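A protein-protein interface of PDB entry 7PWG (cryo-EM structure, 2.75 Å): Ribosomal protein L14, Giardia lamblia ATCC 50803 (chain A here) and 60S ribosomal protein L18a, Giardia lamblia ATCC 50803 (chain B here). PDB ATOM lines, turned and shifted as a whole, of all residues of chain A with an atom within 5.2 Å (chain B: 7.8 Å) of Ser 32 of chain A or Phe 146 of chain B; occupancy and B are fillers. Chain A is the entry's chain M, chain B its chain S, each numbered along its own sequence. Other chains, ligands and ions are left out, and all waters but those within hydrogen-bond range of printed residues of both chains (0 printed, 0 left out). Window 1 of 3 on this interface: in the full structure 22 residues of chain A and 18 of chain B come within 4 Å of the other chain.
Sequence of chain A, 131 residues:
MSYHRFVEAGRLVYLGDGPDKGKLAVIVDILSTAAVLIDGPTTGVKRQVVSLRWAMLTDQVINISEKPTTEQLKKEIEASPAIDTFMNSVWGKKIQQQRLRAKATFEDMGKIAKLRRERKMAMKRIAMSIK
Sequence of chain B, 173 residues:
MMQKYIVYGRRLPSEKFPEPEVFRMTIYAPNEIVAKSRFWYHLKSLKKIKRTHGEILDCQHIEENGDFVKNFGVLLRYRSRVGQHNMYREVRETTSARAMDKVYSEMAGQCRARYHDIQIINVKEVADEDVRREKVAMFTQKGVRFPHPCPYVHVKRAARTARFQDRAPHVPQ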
ATOM      1  N   ARG A   5      35.942  14.736   9.666  1.00  0.00           N
ATOM      2  CA  ARG A   5      35.736  15.877   8.782  1.00  0.00           C
ATOM      3  C   ARG A   5      34.739  15.491   7.698  1.00  0.00           C
ATOM      4  O   ARG A   5      34.908  14.467   7.032  1.00  0.00           O
ATOM      5  CB  ARG A   5      37.060  16.341   8.175  1.00  0.00           C
ATOM      6  CG  ARG A   5      38.059  16.812   9.214  1.00  0.00           C
ATOM      7  CD  ARG A   5      39.410  17.114   8.641  1.00  0.00           C
ATOM      8  NE  ARG A   5      40.340  17.511   9.691  1.00  0.00           N
ATOM      9  CZ  ARG A   5      41.634  17.727   9.507  1.00  0.00           C
ATOM     10  NH1 ARG A   5      42.166  17.586   8.311  1.00  0.00           N
ATOM     11  NH2 ARG A   5      42.394  18.077  10.525  1.00  0.00           N
ATOM     12  N   PHE A   6      33.693  16.299   7.541  1.00  0.00           N
ATOM     13  CA  PHE A   6      32.577  15.998   6.654  1.00  0.00           C
ATOM     14  C   PHE A   6      32.304  17.175   5.729  1.00  0.00           C
ATOM     15  O   PHE A   6      32.552  18.327   6.076  1.00  0.00           O
ATOM     16  CB  PHE A   6      31.290  15.671   7.449  1.00  0.00           C
ATOM     17  CG  PHE A   6      31.245  14.270   7.988  1.00  0.00           C
ATOM     18  CD1 PHE A   6      30.738  13.238   7.225  1.00  0.00           C
ATOM     19  CD2 PHE A   6      31.691  13.989   9.259  1.00  0.00           C
ATOM     20  CE1 PHE A   6      30.691  11.957   7.718  1.00  0.00           C
ATOM     21  CE2 PHE A   6      31.648  12.702   9.755  1.00  0.00           C
ATOM     22  CZ  PHE A   6      31.155  11.689   8.980  1.00  0.00           C
ATOM     23  N   VAL A   7      31.803  16.865   4.538  1.00  0.00           N
ATOM     24  CA  VAL A   7      31.310  17.874   3.608  1.00  0.00           C
ATOM     25  C   VAL A   7      29.900  18.255   4.032  1.00  0.00           C
ATOM     26  O   VAL A   7      29.004  17.407   4.080  1.00  0.00           O
ATOM     27  CB  VAL A   7      31.321  17.353   2.162  1.00  0.00           C
ATOM     28  CG1 VAL A   7      30.980  18.465   1.191  1.00  0.00           C
ATOM     29  CG2 VAL A   7      32.642  16.765   1.825  1.00  0.00           C
ATOM     30  N   ILE A  30      25.592  22.170  -1.715  1.00  0.00           N
ATOM     31  CA  ILE A  30      26.168  20.899  -2.153  1.00  0.00           C
ATOM     32  C   ILE A  30      25.460  20.486  -3.434  1.00  0.00           C
ATOM     33  O   ILE A  30      24.336  19.979  -3.393  1.00  0.00           O
ATOM     34  CB  ILE A  30      26.043  19.805  -1.090  1.00  0.00           C
ATOM     35  CG1 ILE A  30      26.506  20.317   0.270  1.00  0.00           C
ATOM     36  CG2 ILE A  30      26.856  18.587  -1.498  1.00  0.00           C
ATOM     37  CD1 ILE A  30      27.955  20.646   0.321  1.00  0.00           C
ATOM     38  N   LEU A  31      26.104  20.701  -4.578  1.00  0.00           N
ATOM     39  CA  LEU A  31      25.496  20.288  -5.838  1.00  0.00           C
ATOM     40  C   LEU A  31      25.414  18.769  -5.940  1.00  0.00           C
ATOM     41  O   LEU A  31      24.347  18.215  -6.209  1.00  0.00           O
ATOM     42  CB  LEU A  31      26.273  20.872  -7.014  1.00  0.00           C
ATOM     43  CG  LEU A  31      26.020  22.334  -7.391  1.00  0.00           C
ATOM     44  CD1 LEU A  31      26.568  23.317  -6.357  1.00  0.00           C
ATOM     45  CD2 LEU A  31      26.607  22.600  -8.752  1.00  0.00           C
ATOM     46  N   SER A  32      26.520  18.080  -5.711  1.00  0.00           N
ATOM     47  CA  SER A  32      26.573  16.626  -5.810  1.00  0.00           C
ATOM     48  C   SER A  32      27.841  16.160  -5.114  1.00  0.00           C
ATOM     49  O   SER A  32      28.466  16.914  -4.366  1.00  0.00           O
ATOM     50  CB  SER A  32      26.498  16.171  -7.266  1.00  0.00           C
ATOM     51  OG  SER A  32      27.586  16.667  -8.022  1.00  0.00           O
ATOM     52  N   THR A  33      28.217  14.912  -5.339  1.00  0.00           N
ATOM     53  CA  THR A  33      29.472  14.410  -4.799  1.00  0.00           C
ATOM     54  C   THR A  33      30.692  14.877  -5.587  1.00  0.00           C
ATOM     55  O   THR A  33      31.800  14.433  -5.293  1.00  0.00           O
ATOM     56  CB  THR A  33      29.457  12.886  -4.732  1.00  0.00           C
ATOM     57  OG1 THR A  33      29.022  12.346  -5.987  1.00  0.00           O
ATOM     58  CG2 THR A  33      28.530  12.412  -3.627  1.00  0.00           C
ATOM     59  N   ALA A  34      30.529  15.767  -6.563  1.00  0.00           N
ATOM     60  CA  ALA A  34      31.672  16.307  -7.282  1.00  0.00           C
ATOM     61  C   ALA A  34      31.943  17.779  -7.026  1.00  0.00           C
ATOM     62  O   ALA A  34      33.069  18.217  -7.261  1.00  0.00           O
ATOM     63  CB  ALA A  34      31.505  16.110  -8.794  1.00  0.00           C
ATOM     64  N   ALA A  35      30.960  18.556  -6.579  1.00  0.00           N
ATOM     65  CA  ALA A  35      31.099  20.002  -6.597  1.00  0.00           C
ATOM     66  C   ALA A  35      30.307  20.635  -5.464  1.00  0.00           C
ATOM     67  O   ALA A  35      29.349  20.058  -4.948  1.00  0.00           O
ATOM     68  CB  ALA A  35      30.642  20.580  -7.934  1.00  0.00           C
ATOM     69  N   LEU A  52      35.252  19.401  -5.754  1.00  0.00           N
ATOM     70  CA  LEU A  52      35.712  18.930  -4.454  1.00  0.00           C
ATOM     71  C   LEU A  52      37.154  18.437  -4.488  1.00  0.00           C
ATOM     72  O   LEU A  52      37.802  18.387  -3.441  1.00  0.00           O
ATOM     73  CB  LEU A  52      34.772  17.847  -3.927  1.00  0.00           C
ATOM     74  CG  LEU A  52      33.640  18.420  -3.061  1.00  0.00           C
ATOM     75  CD1 LEU A  52      32.535  17.431  -2.865  1.00  0.00           C
ATOM     76  CD2 LEU A  52      34.169  18.867  -1.721  1.00  0.00           C
ATOM     77  N   VAL B  69      21.539  27.381  -5.854  1.00  0.00           N
ATOM     78  CA  VAL B  69      21.604  26.086  -6.529  1.00  0.00           C
ATOM     79  C   VAL B  69      20.194  25.554  -6.715  1.00  0.00           C
ATOM     80  O   VAL B  69      19.476  25.315  -5.738  1.00  0.00           O
ATOM     81  CB  VAL B  69      22.464  25.091  -5.735  1.00  0.00           C
ATOM     82  CG1 VAL B  69      22.517  23.729  -6.428  1.00  0.00           C
ATOM     83  CG2 VAL B  69      23.859  25.652  -5.540  1.00  0.00           C
ATOM     84  N   ARG B  92      21.676  19.326 -10.922  1.00  0.00           N
ATOM     85  CA  ARG B  92      21.692  20.473 -10.027  1.00  0.00           C
ATOM     86  C   ARG B  92      22.817  21.401 -10.446  1.00  0.00           C
ATOM     87  O   ARG B  92      23.978  20.986 -10.483  1.00  0.00           O
ATOM     88  CB  ARG B  92      21.871  20.048  -8.574  1.00  0.00           C
ATOM     89  CG  ARG B  92      20.609  19.578  -7.923  1.00  0.00           C
ATOM     90  CD  ARG B  92      20.843  19.183  -6.483  1.00  0.00           C
ATOM     91  NE  ARG B  92      20.312  20.158  -5.541  1.00  0.00           N
ATOM     92  CZ  ARG B  92      21.055  20.832  -4.675  1.00  0.00           C
ATOM     93  NH1 ARG B  92      22.358  20.628  -4.627  1.00  0.00           N
ATOM     94  NH2 ARG B  92      20.493  21.691  -3.847  1.00  0.00           N
ATOM     95  N   GLU B  93      22.480  22.654 -10.736  1.00  0.00           N
ATOM     96  CA  GLU B  93      23.469  23.651 -11.116  1.00  0.00           C
ATOM     97  C   GLU B  93      22.954  25.027 -10.728  1.00  0.00           C
ATOM     98  O   GLU B  93      21.890  25.170 -10.128  1.00  0.00           O
ATOM     99  CB  GLU B  93      23.794  23.598 -12.616  1.00  0.00           C
ATOM    100  CG  GLU B  93      24.948  22.699 -13.001  1.00  0.00           C
ATOM    101  CD  GLU B  93      26.319  23.227 -12.581  1.00  0.00           C
ATOM    102  OE1 GLU B  93      26.429  24.400 -12.187  1.00  0.00           O
ATOM    103  OE2 GLU B  93      27.299  22.457 -12.655  1.00  0.00           O
ATOM    104  N   LYS B 102      26.684  20.412 -18.025  1.00  0.00           N
ATOM    105  CA  LYS B 102      26.706  19.132 -17.337  1.00  0.00           C
ATOM    106  C   LYS B 102      26.026  18.056 -18.165  1.00  0.00           C
ATOM    107  O   LYS B 102      26.498  16.919 -18.220  1.00  0.00           O
ATOM    108  CB  LYS B 102      26.052  19.263 -15.965  1.00  0.00           C
ATOM    109  CG  LYS B 102      26.129  18.008 -15.100  1.00  0.00           C
ATOM    110  CD  LYS B 102      27.503  17.827 -14.477  1.00  0.00           C
ATOM    111  CE  LYS B 102      27.600  16.515 -13.702  1.00  0.00           C
ATOM    112  NZ  LYS B 102      28.924  16.285 -13.093  1.00  0.00           N
ATOM    113  N   GLU B 106      27.708  14.408 -19.815  1.00  0.00           N
ATOM    114  CA  GLU B 106      27.188  13.094 -19.463  1.00  0.00           C
ATOM    115  C   GLU B 106      26.724  12.316 -20.688  1.00  0.00           C
ATOM    116  O   GLU B 106      26.819  11.087 -20.717  1.00  0.00           O
ATOM    117  CB  GLU B 106      26.042  13.233 -18.470  1.00  0.00           C
ATOM    118  CG  GLU B 106      26.480  13.598 -17.080  1.00  0.00           C
ATOM    119  CD  GLU B 106      25.334  14.096 -16.215  1.00  0.00           C
ATOM    120  OE1 GLU B 106      24.159  13.937 -16.610  1.00  0.00           O
ATOM    121  OE2 GLU B 106      25.610  14.657 -15.135  1.00  0.00           O
ATOM    122  N   LYS B 135      19.709  10.383  -7.840  1.00  0.00           N
ATOM    123  CA  LYS B 135      20.978  11.070  -7.643  1.00  0.00           C
ATOM    124  C   LYS B 135      20.761  12.523  -7.243  1.00  0.00           C
ATOM    125  O   LYS B 135      21.323  12.996  -6.252  1.00  0.00           O
ATOM    126  CB  LYS B 135      21.801  10.976  -8.921  1.00  0.00           C
ATOM    127  CG  LYS B 135      23.277  10.867  -8.723  1.00  0.00           C
ATOM    128  CD  LYS B 135      23.987  10.771 -10.066  1.00  0.00           C
ATOM    129  CE  LYS B 135      23.835   9.404 -10.682  1.00  0.00           C
ATOM    130  NZ  LYS B 135      24.456   8.338  -9.869  1.00  0.00           N
ATOM    131  N   VAL B 136      19.922  13.237  -7.994  1.00  0.00           N
ATOM    132  CA  VAL B 136      19.599  14.621  -7.672  1.00  0.00           C
ATOM    133  C   VAL B 136      18.918  14.707  -6.315  1.00  0.00           C
ATOM    134  O   VAL B 136      19.327  15.481  -5.446  1.00  0.00           O
ATOM    135  CB  VAL B 136      18.716  15.220  -8.783  1.00  0.00           C
ATOM    136  CG1 VAL B 136      18.213  16.593  -8.402  1.00  0.00           C
ATOM    137  CG2 VAL B 136      19.461  15.256 -10.090  1.00  0.00           C
ATOM    138  N   MET B 138      18.912  13.097  -3.561  1.00  0.00           N
ATOM    139  CA  MET B 138      19.700  12.968  -2.339  1.00  0.00           C
ATOM    140  C   MET B 138      20.096  14.327  -1.778  1.00  0.00           C
ATOM    141  O   MET B 138      20.105  14.528  -0.561  1.00  0.00           O
ATOM    142  CB  MET B 138      20.958  12.145  -2.608  1.00  0.00           C
ATOM    143  CG  MET B 138      20.756  10.652  -2.641  1.00  0.00           C
ATOM    144  SD  MET B 138      21.919   9.806  -3.734  1.00  0.00           S
ATOM    145  CE  MET B 138      23.422  10.678  -3.391  1.00  0.00           C
ATOM    146  N   PHE B 139      20.432  15.267  -2.652  1.00  0.00           N
ATOM    147  CA  PHE B 139      20.956  16.552  -2.234  1.00  0.00           C
ATOM    148  C   PHE B 139      19.881  17.619  -2.085  1.00  0.00           C
ATOM    149  O   PHE B 139      20.189  18.718  -1.616  1.00  0.00           O
ATOM    150  CB  PHE B 139      22.030  17.006  -3.224  1.00  0.00           C
ATOM    151  CG  PHE B 139      23.118  15.999  -3.437  1.00  0.00           C
ATOM    152  CD1 PHE B 139      23.009  15.035  -4.423  1.00  0.00           C
ATOM    153  CD2 PHE B 139      24.252  16.014  -2.654  1.00  0.00           C
ATOM    154  CE1 PHE B 139      24.009  14.114  -4.611  1.00  0.00           C
ATOM    155  CE2 PHE B 139      25.248  15.094  -2.838  1.00  0.00           C
ATOM    156  CZ  PHE B 139      25.132  14.148  -3.812  1.00  0.00           C
ATOM    157  N   GLY B 143      20.482  19.088   5.727  1.00  0.00           N
ATOM    158  CA  GLY B 143      21.486  18.463   6.566  1.00  0.00           C
ATOM    159  C   GLY B 143      22.309  17.368   5.934  1.00  0.00           C
ATOM    160  O   GLY B 143      22.842  16.529   6.662  1.00  0.00           O
ATOM    161  N   VAL B 144      22.446  17.342   4.609  1.00  0.00           N
ATOM    162  CA  VAL B 144      23.195  16.266   3.971  1.00  0.00           C
ATOM    163  C   VAL B 144      24.673  16.387   4.333  1.00  0.00           C
ATOM    164  O   VAL B 144      25.273  17.462   4.229  1.00  0.00           O
ATOM    165  CB  VAL B 144      22.955  16.269   2.450  1.00  0.00           C
ATOM    166  CG1 VAL B 144      23.598  17.446   1.777  1.00  0.00           C
ATOM    167  CG2 VAL B 144      23.441  14.981   1.820  1.00  0.00           C
ATOM    168  N   ARG B 145      25.254  15.291   4.815  1.00  0.00           N
ATOM    169  CA  ARG B 145      26.672  15.219   5.139  1.00  0.00           C
ATOM    170  C   ARG B 145      27.265  13.960   4.547  1.00  0.00           C
ATOM    171  O   ARG B 145      26.637  12.898   4.561  1.00  0.00           O
ATOM    172  CB  ARG B 145      26.956  15.184   6.631  1.00  0.00           C
ATOM    173  CG  ARG B 145      26.010  15.936   7.505  1.00  0.00           C
ATOM    174  CD  ARG B 145      26.744  16.410   8.752  1.00  0.00           C
ATOM    175  NE  ARG B 145      27.069  15.313   9.656  1.00  0.00           N
ATOM    176  CZ  ARG B 145      28.150  15.277  10.426  1.00  0.00           C
ATOM    177  NH1 ARG B 145      29.022  16.273  10.385  1.00  0.00           N
ATOM    178  NH2 ARG B 145      28.371  14.244  11.217  1.00  0.00           N
ATOM    179  N   PHE B 146      28.480  14.079   4.041  1.00  0.00           N
ATOM    180  CA  PHE B 146      29.260  12.918   3.662  1.00  0.00           C
ATOM    181  C   PHE B 146      30.720  13.236   3.906  1.00  0.00           C
ATOM    182  O   PHE B 146      31.098  14.408   3.989  1.00  0.00           O
ATOM    183  CB  PHE B 146      29.019  12.509   2.203  1.00  0.00           C
ATOM    184  CG  PHE B 146      28.963  13.653   1.234  1.00  0.00           C
ATOM    185  CD1 PHE B 146      27.800  14.372   1.063  1.00  0.00           C
ATOM    186  CD2 PHE B 146      30.061  13.976   0.461  1.00  0.00           C
ATOM    187  CE1 PHE B 146      27.742  15.408   0.169  1.00  0.00           C
ATOM    188  CE2 PHE B 146      30.002  15.023  -0.438  1.00  0.00           C
ATOM    189  CZ  PHE B 146      28.843  15.732  -0.585  1.00  0.00           C
ATOM    190  N   PRO B 147      31.552  12.225   4.089  1.00  0.00           N
ATOM    191  CA  PRO B 147      32.990  12.464   4.155  1.00  0.00           C
ATOM    192  C   PRO B 147      33.554  12.679   2.762  1.00  0.00           C
ATOM    193  O   PRO B 147      32.911  12.385   1.758  1.00  0.00           O
ATOM    194  CB  PRO B 147      33.533  11.189   4.800  1.00  0.00           C
ATOM    195  CG  PRO B 147      32.540  10.165   4.508  1.00  0.00           C
ATOM    196  CD  PRO B 147      31.202  10.826   4.376  1.00  0.00           C
ATOM    197  N   HIS B 148      34.765  13.220   2.714  1.00  0.00           N
ATOM    198  CA  HIS B 148      35.330  13.640   1.442  1.00  0.00           C
ATOM    199  C   HIS B 148      35.417  12.447   0.497  1.00  0.00           C
ATOM    200  O   HIS B 148      35.970  11.407   0.870  1.00  0.00           O
ATOM    201  CB  HIS B 148      36.708  14.260   1.643  1.00  0.00           C
ATOM    202  CG  HIS B 148      37.151  15.149   0.523  1.00  0.00           C
ATOM    203  ND1 HIS B 148      37.080  14.781  -0.802  1.00  0.00           N
ATOM    204  CD2 HIS B 148      37.696  16.386   0.535  1.00  0.00           C
ATOM    205  CE1 HIS B 148      37.551  15.755  -1.556  1.00  0.00           C
ATOM    206  NE2 HIS B 148      37.934  16.740  -0.770  1.00  0.00           N
ATOM    207  N   PRO B 149      34.872  12.542  -0.716  1.00  0.00           N
ATOM    208  CA  PRO B 149      34.847  11.374  -1.604  1.00  0.00           C
ATOM    209  C   PRO B 149      36.170  11.027  -2.265  1.00  0.00           C
ATOM    210  O   PRO B 149      36.240   9.980  -2.917  1.00  0.00           O
ATOM    211  CB  PRO B 149      33.790  11.757  -2.648  1.00  0.00           C
ATOM    212  CG  PRO B 149      33.713  13.218  -2.596  1.00  0.00           C
ATOM    213  CD  PRO B 149      34.002  13.620  -1.204  1.00  0.00           C
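N of Val 7 of chain A lies within hydrogen-bond range of O of Phe 146 of chain B (2.6 Å).
NH1 of Arg 92 of chain B sits at hydrogen-bond distance from O of Ile 30 of chain A, at 2.4 Å.
The backbone carbonyl oxygen (O) of Leu 52 of chain A lies within hydrogen-bond range of a ring nitrogen (NE2) of His 148 of chain B (3.1 Å).
Ser 32 of chain A touches two residues of chain B.
Phe 146 of chain B touches just these residues of chain A: Phe 6, Val 7, Ile 30 and Ser 32.
Of the printed residues of chain B, Val 7 of chain A touches Val 144, Arg 145 and Phe 146.
Printed residues of chain A within 4 Å of Pro 147 of chain B: Arg 5 and Phe 6.
Met 138 of chain B touches none of the printed residues of chain A.
The nearest printed residue of chain A that does not touch Pro 147 of chain B is Val 7 of chain A (4.3 Å).
Arg 5 of chain A touches Pro 147 of chain B (O to CA, 3.996 Å).
Arg 145 of chain B touches Phe 6 of chain A (NH1 to CD2, 3.7 Å).
Phe 146 of chain B touches Phe 6 of chain A.
O of Val 7 of chain A touches O of Val 144 of chain B (3.7 Å).
Arg 145 of chain B touches Val 7 of chain A (CA to O, 3.4 Å).
Phe 146 of chain B touches Ile 30 of chain A (CZ to CG2, 3.6 Å).
CD1 of Leu 31 of chain A touches CG2 of Val 69 of chain B (3.7 Å).
Arg 92 of chain B touches Leu 31 of chain A (NH1 to CA, 3.4 Å).
Leu 31 of chain A touches Glu 93 of chain B.
Thr 33 of chain A touches Phe 139 of chain B.
Hydrophobic or aromatic side chains of chain A within 4 Å of the printed part of chain B: Phe 6, Val 7, Ile 30 and Leu 31.
Among the printed residues, 19 pairs touch across the chains.
Among the printed residues, no Asp or Glu carboxylate lies within 4 Å of a Lys or Arg side-chain nitrogen of the other chain.
The backbone NH (N) of Ala 34 of chain A lies close to the side-chain hydroxyl (OG) of Ser 32 of chain A, at 3.4 Å.
The backbone NH (N) of Leu 52 of chain A lies within hydrogen-bond range of the backbone carbonyl oxygen (O) of Ala 34 of chain A (2.9 Å).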
